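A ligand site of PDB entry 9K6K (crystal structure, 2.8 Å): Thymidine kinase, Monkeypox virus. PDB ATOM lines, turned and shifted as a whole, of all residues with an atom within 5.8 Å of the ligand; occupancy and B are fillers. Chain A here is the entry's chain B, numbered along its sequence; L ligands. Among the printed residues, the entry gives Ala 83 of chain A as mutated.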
ATOM      1  N   PRO A  12       6.795  27.580  32.001  1.00  0.00           N
ATOM      2  CA  PRO A  12       8.237  27.408  31.827  1.00  0.00           C
ATOM      3  C   PRO A  12       8.538  26.055  31.229  1.00  0.00           C
ATOM      4  O   PRO A  12       7.637  25.254  30.971  1.00  0.00           O
ATOM      5  CB  PRO A  12       8.773  27.520  33.257  1.00  0.00           C
ATOM      6  CG  PRO A  12       7.649  27.012  34.089  1.00  0.00           C
ATOM      7  CD  PRO A  12       6.398  27.502  33.416  1.00  0.00           C
ATOM      8  N   MET A  13       9.817  25.801  30.981  1.00  0.00           N
ATOM      9  CA  MET A  13      10.225  24.474  30.577  1.00  0.00           C
ATOM     10  C   MET A  13       9.914  23.507  31.706  1.00  0.00           C
ATOM     11  O   MET A  13       9.857  23.879  32.882  1.00  0.00           O
ATOM     12  CB  MET A  13      11.709  24.455  30.247  1.00  0.00           C
ATOM     13  CG  MET A  13      12.085  25.390  29.123  1.00  0.00           C
ATOM     14  SD  MET A  13      13.778  25.125  28.569  1.00  0.00           S
ATOM     15  CE  MET A  13      13.751  23.358  28.260  1.00  0.00           C
ATOM     16  N   PHE A  14       9.719  22.250  31.337  1.00  0.00           N
ATOM     17  CA  PHE A  14       9.471  21.148  32.255  1.00  0.00           C
ATOM     18  C   PHE A  14       8.138  21.277  33.004  1.00  0.00           C
ATOM     19  O   PHE A  14       7.959  20.635  34.032  1.00  0.00           O
ATOM     20  CB  PHE A  14      10.628  21.012  33.253  1.00  0.00           C
ATOM     21  CG  PHE A  14      11.974  21.217  32.630  1.00  0.00           C
ATOM     22  CD1 PHE A  14      12.484  20.283  31.734  1.00  0.00           C
ATOM     23  CD2 PHE A  14      12.735  22.340  32.919  1.00  0.00           C
ATOM     24  CE1 PHE A  14      13.726  20.455  31.143  1.00  0.00           C
ATOM     25  CE2 PHE A  14      13.977  22.526  32.345  1.00  0.00           C
ATOM     26  CZ  PHE A  14      14.480  21.580  31.448  1.00  0.00           C
ATOM     27  N   SER A  15       7.195  22.075  32.499  1.00  0.00           N
ATOM     28  CA  SER A  15       5.885  22.170  33.148  1.00  0.00           C
ATOM     29  C   SER A  15       4.825  21.266  32.511  1.00  0.00           C
ATOM     30  O   SER A  15       3.727  21.163  33.051  1.00  0.00           O
ATOM     31  CB  SER A  15       5.389  23.627  33.163  1.00  0.00           C
ATOM     32  OG  SER A  15       5.305  24.198  31.868  1.00  0.00           O
ATOM     33  N   GLY A  16       5.126  20.633  31.374  1.00  0.00           N
ATOM     34  CA  GLY A  16       4.203  19.710  30.754  1.00  0.00           C
ATOM     35  C   GLY A  16       3.323  20.280  29.656  1.00  0.00           C
ATOM     36  O   GLY A  16       2.281  19.686  29.367  1.00  0.00           O
ATOM     37  N   LYS A  17       3.726  21.401  29.026  1.00  0.00           N
ATOM     38  CA  LYS A  17       2.904  22.035  28.000  1.00  0.00           C
ATOM     39  C   LYS A  17       2.623  21.085  26.834  1.00  0.00           C
ATOM     40  O   LYS A  17       1.487  20.979  26.372  1.00  0.00           O
ATOM     41  CB  LYS A  17       3.592  23.294  27.465  1.00  0.00           C
ATOM     42  CG  LYS A  17       3.837  24.375  28.498  1.00  0.00           C
ATOM     43  CD  LYS A  17       4.490  25.617  27.876  1.00  0.00           C
ATOM     44  CE  LYS A  17       5.852  25.318  27.274  1.00  0.00           C
ATOM     45  NZ  LYS A  17       6.783  24.822  28.321  1.00  0.00           N
ATOM     46  N   SER A  18       3.648  20.373  26.368  1.00  0.00           N
ATOM     47  CA  SER A  18       3.477  19.504  25.217  1.00  0.00           C
ATOM     48  C   SER A  18       2.534  18.339  25.514  1.00  0.00           C
ATOM     49  O   SER A  18       1.726  17.952  24.654  1.00  0.00           O
ATOM     50  CB  SER A  18       4.841  19.010  24.753  1.00  0.00           C
ATOM     51  OG  SER A  18       5.569  18.464  25.852  1.00  0.00           O
ATOM     52  N   THR A  19       2.621  17.778  26.723  1.00  0.00           N
ATOM     53  CA  THR A  19       1.727  16.682  27.094  1.00  0.00           C
ATOM     54  C   THR A  19       0.287  17.154  27.184  1.00  0.00           C
ATOM     55  O   THR A  19      -0.634  16.458  26.733  1.00  0.00           O
ATOM     56  CB  THR A  19       2.187  16.071  28.414  1.00  0.00           C
ATOM     57  OG1 THR A  19       3.541  15.624  28.271  1.00  0.00           O
ATOM     58  CG2 THR A  19       1.310  14.897  28.794  1.00  0.00           C
ATOM     59  N   ASP A  43      14.372  20.290  16.774  1.00  0.00           N
ATOM     60  CA  ASP A  43      14.158  20.644  18.177  1.00  0.00           C
ATOM     61  C   ASP A  43      15.293  20.115  19.051  1.00  0.00           C
ATOM     62  O   ASP A  43      15.817  20.841  19.905  1.00  0.00           O
ATOM     63  CB  ASP A  43      12.808  20.112  18.652  1.00  0.00           C
ATOM     64  CG  ASP A  43      12.361  20.727  19.971  1.00  0.00           C
ATOM     65  OD1 ASP A  43      12.649  21.920  20.214  1.00  0.00           O
ATOM     66  OD2 ASP A  43      11.708  20.021  20.767  1.00  0.00           O
ATOM     67  N   ASP A  82       3.295  22.862  18.681  1.00  0.00           N
ATOM     68  CA  ASP A  82       4.243  22.767  19.774  1.00  0.00           C
ATOM     69  C   ASP A  82       5.458  23.646  19.498  1.00  0.00           C
ATOM     70  O   ASP A  82       5.904  23.775  18.352  1.00  0.00           O
ATOM     71  CB  ASP A  82       4.679  21.321  20.014  1.00  0.00           C
ATOM     72  CG  ASP A  82       5.238  21.099  21.400  1.00  0.00           C
ATOM     73  OD1 ASP A  82       5.625  22.085  22.057  1.00  0.00           O
ATOM     74  OD2 ASP A  82       5.277  19.934  21.844  1.00  0.00           O
ATOM     75  N   ALA A  83       5.993  24.238  20.569  1.00  0.00           N
ATOM     76  CA  ALA A  83       7.073  25.215  20.492  1.00  0.00           C
ATOM     77  C   ALA A  83       6.701  26.364  19.555  1.00  0.00           C
ATOM     78  O   ALA A  83       7.450  26.767  18.664  1.00  0.00           O
ATOM     79  CB  ALA A  83       8.384  24.550  20.056  1.00  0.00           C
ATOM     80  N   GLN A  85       6.538  29.519  20.003  1.00  0.00           N
ATOM     81  CA  GLN A  85       7.265  30.789  20.096  1.00  0.00           C
ATOM     82  C   GLN A  85       8.289  30.953  18.988  1.00  0.00           C
ATOM     83  O   GLN A  85       8.676  32.090  18.673  1.00  0.00           O
ATOM     84  CB  GLN A  85       7.974  30.913  21.449  1.00  0.00           C
ATOM     85  CG  GLN A  85       9.125  29.944  21.660  1.00  0.00           C
ATOM     86  CD  GLN A  85       8.649  28.583  22.107  1.00  0.00           C
ATOM     87  OE1 GLN A  85       7.447  28.376  22.338  1.00  0.00           O
ATOM     88  NE2 GLN A  85       9.569  27.630  22.190  1.00  0.00           N
ATOM     89  N   PHE A  86       8.752  29.851  18.377  1.00  0.00           N
ATOM     90  CA  PHE A  86       9.752  29.923  17.325  1.00  0.00           C
ATOM     91  C   PHE A  86       9.182  30.370  15.986  1.00  0.00           C
ATOM     92  O   PHE A  86       9.946  30.858  15.142  1.00  0.00           O
ATOM     93  CB  PHE A  86      10.420  28.557  17.148  1.00  0.00           C
ATOM     94  CG  PHE A  86      11.229  28.125  18.341  1.00  0.00           C
ATOM     95  CD1 PHE A  86      11.963  29.042  19.057  1.00  0.00           C
ATOM     96  CD2 PHE A  86      11.236  26.803  18.740  1.00  0.00           C
ATOM     97  CE1 PHE A  86      12.705  28.647  20.152  1.00  0.00           C
ATOM     98  CE2 PHE A  86      11.975  26.400  19.840  1.00  0.00           C
ATOM     99  CZ  PHE A  86      12.715  27.316  20.540  1.00  0.00           C
ATOM    100  N   ALA A 108       3.394  27.018  24.059  1.00  0.00           N
ATOM    101  CA  ALA A 108       4.550  27.879  23.818  1.00  0.00           C
ATOM    102  C   ALA A 108       5.148  28.351  25.130  1.00  0.00           C
ATOM    103  O   ALA A 108       4.545  28.220  26.191  1.00  0.00           O
ATOM    104  CB  ALA A 108       4.156  29.097  22.959  1.00  0.00           C
ATOM    105  N   LEU A 109       6.371  28.876  25.042  1.00  0.00           N
ATOM    106  CA  LEU A 109       7.016  29.516  26.187  1.00  0.00           C
ATOM    107  C   LEU A 109       6.604  30.979  26.277  1.00  0.00           C
ATOM    108  O   LEU A 109       6.572  31.697  25.272  1.00  0.00           O
ATOM    109  CB  LEU A 109       8.539  29.428  26.084  1.00  0.00           C
ATOM    110  CG  LEU A 109       9.271  28.129  26.435  1.00  0.00           C
ATOM    111  CD1 LEU A 109      10.754  28.321  26.220  1.00  0.00           C
ATOM    112  CD2 LEU A 109       8.992  27.696  27.851  1.00  0.00           C
ATOM    113  N   GLY A 111       8.286  33.232  28.345  1.00  0.00           N
ATOM    114  CA  GLY A 111       9.476  34.043  28.520  1.00  0.00           C
ATOM    115  C   GLY A 111      10.745  33.274  28.184  1.00  0.00           C
ATOM    116  O   GLY A 111      10.831  32.057  28.366  1.00  0.00           O
ATOM    117  N   THR A 112      11.755  34.025  27.743  1.00  0.00           N
ATOM    118  CA  THR A 112      13.060  33.467  27.406  1.00  0.00           C
ATOM    119  C   THR A 112      13.837  33.200  28.694  1.00  0.00           C
ATOM    120  O   THR A 112      13.289  33.205  29.800  1.00  0.00           O
ATOM    121  CB  THR A 112      13.803  34.403  26.471  1.00  0.00           C
ATOM    122  OG1 THR A 112      14.212  35.585  27.184  1.00  0.00           O
ATOM    123  CG2 THR A 112      12.914  34.805  25.307  1.00  0.00           C
ATOM    124  N   PHE A 113      15.142  32.947  28.574  1.00  0.00           N
ATOM    125  CA  PHE A 113      15.947  32.733  29.774  1.00  0.00           C
ATOM    126  C   PHE A 113      16.130  34.016  30.570  1.00  0.00           C
ATOM    127  O   PHE A 113      16.457  33.953  31.759  1.00  0.00           O
ATOM    128  CB  PHE A 113      17.327  32.149  29.419  1.00  0.00           C
ATOM    129  CG  PHE A 113      18.211  33.089  28.631  1.00  0.00           C
ATOM    130  CD1 PHE A 113      17.970  33.345  27.289  1.00  0.00           C
ATOM    131  CD2 PHE A 113      19.285  33.695  29.248  1.00  0.00           C
ATOM    132  CE1 PHE A 113      18.790  34.213  26.583  1.00  0.00           C
ATOM    133  CE2 PHE A 113      20.111  34.551  28.546  1.00  0.00           C
ATOM    134  CZ  PHE A 113      19.864  34.808  27.220  1.00  0.00           C
ATOM    135  N   GLN A 114      15.955  35.173  29.926  1.00  0.00           N
ATOM    136  CA  GLN A 114      16.033  36.472  30.581  1.00  0.00           C
ATOM    137  C   GLN A 114      14.667  36.947  31.071  1.00  0.00           C
ATOM    138  O   GLN A 114      14.524  38.131  31.405  1.00  0.00           O
ATOM    139  CB  GLN A 114      16.627  37.510  29.628  1.00  0.00           C
ATOM    140  CG  GLN A 114      18.057  37.248  29.185  1.00  0.00           C
ATOM    141  CD  GLN A 114      19.095  37.888  30.096  1.00  0.00           C
ATOM    142  OE1 GLN A 114      18.759  38.703  30.964  1.00  0.00           O
ATOM    143  NE2 GLN A 114      20.367  37.532  29.899  1.00  0.00           N
ATOM    144  N   PHE A 118       8.991  36.248  24.494  1.00  0.00           N
ATOM    145  CA  PHE A 118       9.561  35.425  23.430  1.00  0.00           C
ATOM    146  C   PHE A 118       8.911  35.771  22.096  1.00  0.00           C
ATOM    147  O   PHE A 118       7.737  35.473  21.875  1.00  0.00           O
ATOM    148  CB  PHE A 118       9.379  33.952  23.759  1.00  0.00           C
ATOM    149  CG  PHE A 118      10.511  33.091  23.299  1.00  0.00           C
ATOM    150  CD1 PHE A 118      11.238  33.414  22.166  1.00  0.00           C
ATOM    151  CD2 PHE A 118      10.886  31.978  24.016  1.00  0.00           C
ATOM    152  CE1 PHE A 118      12.297  32.634  21.745  1.00  0.00           C
ATOM    153  CE2 PHE A 118      11.953  31.182  23.612  1.00  0.00           C
ATOM    154  CZ  PHE A 118      12.656  31.513  22.463  1.00  0.00           C
ATOM    155  N   SER A 148      12.481  29.808  33.476  1.00  0.00           N
ATOM    156  CA  SER A 148      13.510  28.927  32.948  1.00  0.00           C
ATOM    157  C   SER A 148      14.837  29.665  33.040  1.00  0.00           C
ATOM    158  O   SER A 148      14.908  30.863  32.784  1.00  0.00           O
ATOM    159  CB  SER A 148      13.226  28.516  31.496  1.00  0.00           C
ATOM    160  OG  SER A 148      11.946  27.930  31.351  1.00  0.00           O
ATOM    161  N   LYS A 149      15.890  28.927  33.401  1.00  0.00           N
ATOM    162  CA  LYS A 149      17.208  29.517  33.585  1.00  0.00           C
ATOM    163  C   LYS A 149      18.246  28.641  32.917  1.00  0.00           C
ATOM    164  O   LYS A 149      18.344  27.441  33.226  1.00  0.00           O
ATOM    165  CB  LYS A 149      17.543  29.710  35.067  1.00  0.00           C
ATOM    166  CG  LYS A 149      18.903  30.379  35.284  1.00  0.00           C
ATOM    167  CD  LYS A 149      19.115  30.783  36.747  1.00  0.00           C
ATOM    168  CE  LYS A 149      19.176  29.576  37.663  1.00  0.00           C
ATOM    169  NZ  LYS A 149      19.465  29.972  39.082  1.00  0.00           N
ATOM    170  N   GLU A 156      21.158  32.473  24.805  1.00  0.00           N
ATOM    171  CA  GLU A 156      20.172  31.772  23.989  1.00  0.00           C
ATOM    172  C   GLU A 156      18.965  32.641  23.661  1.00  0.00           C
ATOM    173  O   GLU A 156      18.028  32.199  22.993  1.00  0.00           O
ATOM    174  CB  GLU A 156      19.720  30.505  24.696  1.00  0.00           C
ATOM    175  N   ILE A 159      19.710  28.925  21.686  1.00  0.00           N
ATOM    176  CA  ILE A 159      20.236  27.577  21.838  1.00  0.00           C
ATOM    177  C   ILE A 159      19.142  26.683  22.429  1.00  0.00           C
ATOM    178  O   ILE A 159      18.483  27.048  23.394  1.00  0.00           O
ATOM    179  CB  ILE A 159      21.505  27.557  22.712  1.00  0.00           C
ATOM    180  CG1 ILE A 159      22.576  28.490  22.127  1.00  0.00           C
ATOM    181  CG2 ILE A 159      22.058  26.147  22.832  1.00  0.00           C
ATOM    182  CD1 ILE A 159      23.177  27.997  20.811  1.00  0.00           C
ATOM    183  N   ILE A 160      18.939  25.510  21.831  1.00  0.00           N
ATOM    184  CA  ILE A 160      17.913  24.570  22.260  1.00  0.00           C
ATOM    185  C   ILE A 160      18.579  23.460  23.070  1.00  0.00           C
ATOM    186  O   ILE A 160      19.759  23.140  22.897  1.00  0.00           O
ATOM    187  CB  ILE A 160      17.109  23.982  21.081  1.00  0.00           C
ATOM    188  CG1 ILE A 160      17.141  24.921  19.867  1.00  0.00           C
ATOM    189  CG2 ILE A 160      15.675  23.708  21.496  1.00  0.00           C
ATOM    190  CD1 ILE A 160      18.197  24.556  18.836  1.00  0.00           C
ATOM    191  N   GLY A 161      17.804  22.849  23.953  1.00  0.00           N
ATOM    192  CA  GLY A 161      18.324  21.752  24.767  1.00  0.00           C
ATOM    193  C   GLY A 161      17.260  21.235  25.698  1.00  0.00           C
ATOM    194  O   GLY A 161      16.163  21.796  25.810  1.00  0.00           O
ATOM    195  N   GLY A 162      17.591  20.129  26.372  1.00  0.00           N
ATOM    196  CA  GLY A 162      16.698  19.523  27.328  1.00  0.00           C
ATOM    197  C   GLY A 162      16.843  20.118  28.720  1.00  0.00           C
ATOM    198  O   GLY A 162      16.472  21.273  28.939  1.00  0.00           O
ATOM    199  N   TYR A 166      19.310  23.846  30.765  1.00  0.00           N
ATOM    200  CA  TYR A 166      18.230  24.635  31.338  1.00  0.00           C
ATOM    201  C   TYR A 166      17.679  23.958  32.581  1.00  0.00           C
ATOM    202  O   TYR A 166      17.784  22.739  32.752  1.00  0.00           O
ATOM    203  CB  TYR A 166      17.079  24.841  30.348  1.00  0.00           C
ATOM    204  CG  TYR A 166      17.439  25.602  29.098  1.00  0.00           C
ATOM    205  CD1 TYR A 166      17.524  26.997  29.113  1.00  0.00           C
ATOM    206  CD2 TYR A 166      17.661  24.951  27.889  1.00  0.00           C
ATOM    207  CE1 TYR A 166      17.843  27.695  27.965  1.00  0.00           C
ATOM    208  CE2 TYR A 166      17.979  25.650  26.741  1.00  0.00           C
ATOM    209  CZ  TYR A 166      18.075  27.026  26.787  1.00  0.00           C
ATOM    210  OH  TYR A 166      18.390  27.734  25.649  1.00  0.00           O
HETATM  211  P1  LIG L   1       9.925  23.400  25.739  1.00  0.00           P
HETATM  212  O1  LIG L   1       9.607  22.328  24.721  1.00  0.00           O
HETATM  213  O2  LIG L   1       8.775  24.383  25.863  1.00  0.00           O
HETATM  214  O3  LIG L   1      10.258  22.760  27.168  1.00  0.00           O
HETATM  215  P2  LIG L   1       9.911  21.211  27.448  1.00  0.00           P
HETATM  216  O4  LIG L   1       9.195  20.595  26.255  1.00  0.00           O
HETATM  217  O5  LIG L   1      11.180  20.440  27.758  1.00  0.00           O
HETATM  218  O6  LIG L   1       8.966  21.258  28.739  1.00  0.00           O
HETATM  219  P3  LIG L   1       7.439  20.749  28.653  1.00  0.00           P
HETATM  220  O7  LIG L   1       7.230  19.795  27.496  1.00  0.00           O
HETATM  221  O8  LIG L   1       7.097  20.022  29.937  1.00  0.00           O
HETATM  222  O9  LIG L   1       6.533  21.934  28.451  1.00  0.00           O
HETATM  223  O10 LIG L   1      11.280  24.168  25.348  1.00  0.00           O
HETATM  224  C1  LIG L   1      11.373  24.950  24.161  1.00  0.00           C
HETATM  225  C2  LIG L   1      12.835  24.994  23.717  1.00  0.00           C
HETATM  226  O11 LIG L   1      13.269  26.342  23.554  1.00  0.00           O
HETATM  227  C3  LIG L   1      13.745  24.363  24.752  1.00  0.00           C
HETATM  228  O12 LIG L   1      14.143  23.043  24.337  1.00  0.00           O
HETATM  229  C4  LIG L   1      14.958  25.269  24.857  1.00  0.00           C
HETATM  230  C5  LIG L   1      14.633  26.473  23.977  1.00  0.00           C
HETATM  231  N1  LIG L   1      14.820  27.738  24.702  1.00  0.00           N
HETATM  232  C6  LIG L   1      15.241  28.892  23.988  1.00  0.00           C
HETATM  233  O13 LIG L   1      15.448  28.811  22.759  1.00  0.00           O
HETATM  234  N2  LIG L   1      15.429  30.070  24.605  1.00  0.00           N
HETATM  235  C7  LIG L   1      15.222  30.191  25.916  1.00  0.00           C
HETATM  236  O14 LIG L   1      15.387  31.290  26.489  1.00  0.00           O
HETATM  237  C8  LIG L   1      14.776  29.003  26.693  1.00  0.00           C
HETATM  238  C9  LIG L   1      14.532  29.098  28.174  1.00  0.00           C
HETATM  239  C10 LIG L   1      14.594  27.803  26.019  1.00  0.00           C
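OG of Ser 15 lies within hydrogen-bond range of O of Pro 12 (2.7 Å).
OE1 of Gln 85 sits at hydrogen-bond distance from N of Leu 109 (3.0 Å).
The side-chain amino group (NZ) of Lys 17 is in hydrogen-bond range of the backbone carbonyl oxygen (O) of Pro 12 (2.8 Å).
The side-chain hydroxyl (OG) of Ser 148 lies within hydrogen-bond range of the backbone NH (N) of Met 13.
The side-chain hydroxyl (OG1) of Thr 112 sits close to the backbone NH (N) of Gln 114 (3.3 Å).
Met 13 touches the ligand.
Gln 85 touches the ligand.
CZ of Phe 86 touches O11 of the ligand, at 3.2 Å.
Leu 109 touches the ligand.
Thr 112 touches the ligand.
Phe 118 touches the ligand.
Ser 148 touches the ligand (CB to C9, 3.6 Å).
Glu 156 touches the ligand.
Ile 159 touches the ligand (O to O13, 3.6 Å).
Ile 160 touches the ligand (CG2 to O12, 3.3 Å).
Tyr 166 touches the ligand (CE1 to C8, 3.6 Å).
Hydrophobic or aromatic side chains within 4 Å of the ligand: Met 13, Phe 86, Leu 109, Phe 113, Phe 118, Ile 160 and Tyr 166.
The nearest printed residue that does not touch the ligand is Pro 12 (4.3 Å).
N of Phe 14 lies within hydrogen-bond range of O6 of the ligand (2.9 Å).
An oxygen (O12) of the ligand lies within hydrogen-bond range of the backbone carbonyl oxygen (O) of Gly 161, 2.8 Å away.
N of Gly 16 sits at hydrogen-bond distance from O8 of the ligand (2.5 Å).
N of Ser 15 is in hydrogen-bond range of O8 of the ligand, 3.3 Å away.
The backbone NH (N) of Lys 17 sits at hydrogen-bond distance from an oxygen (O9) of the ligand (2.9 Å).
OG of Ser 18 lies within hydrogen-bond range of O7 of the ligand.
An oxygen (O14) of the ligand is in hydrogen-bond range of the backbone NH (N) of Phe 113 (2.7 Å).
The side-chain amino group of Lys 17 lies within salt-bridge range of an oxygen (O9) of the ligand (2.9 Å).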
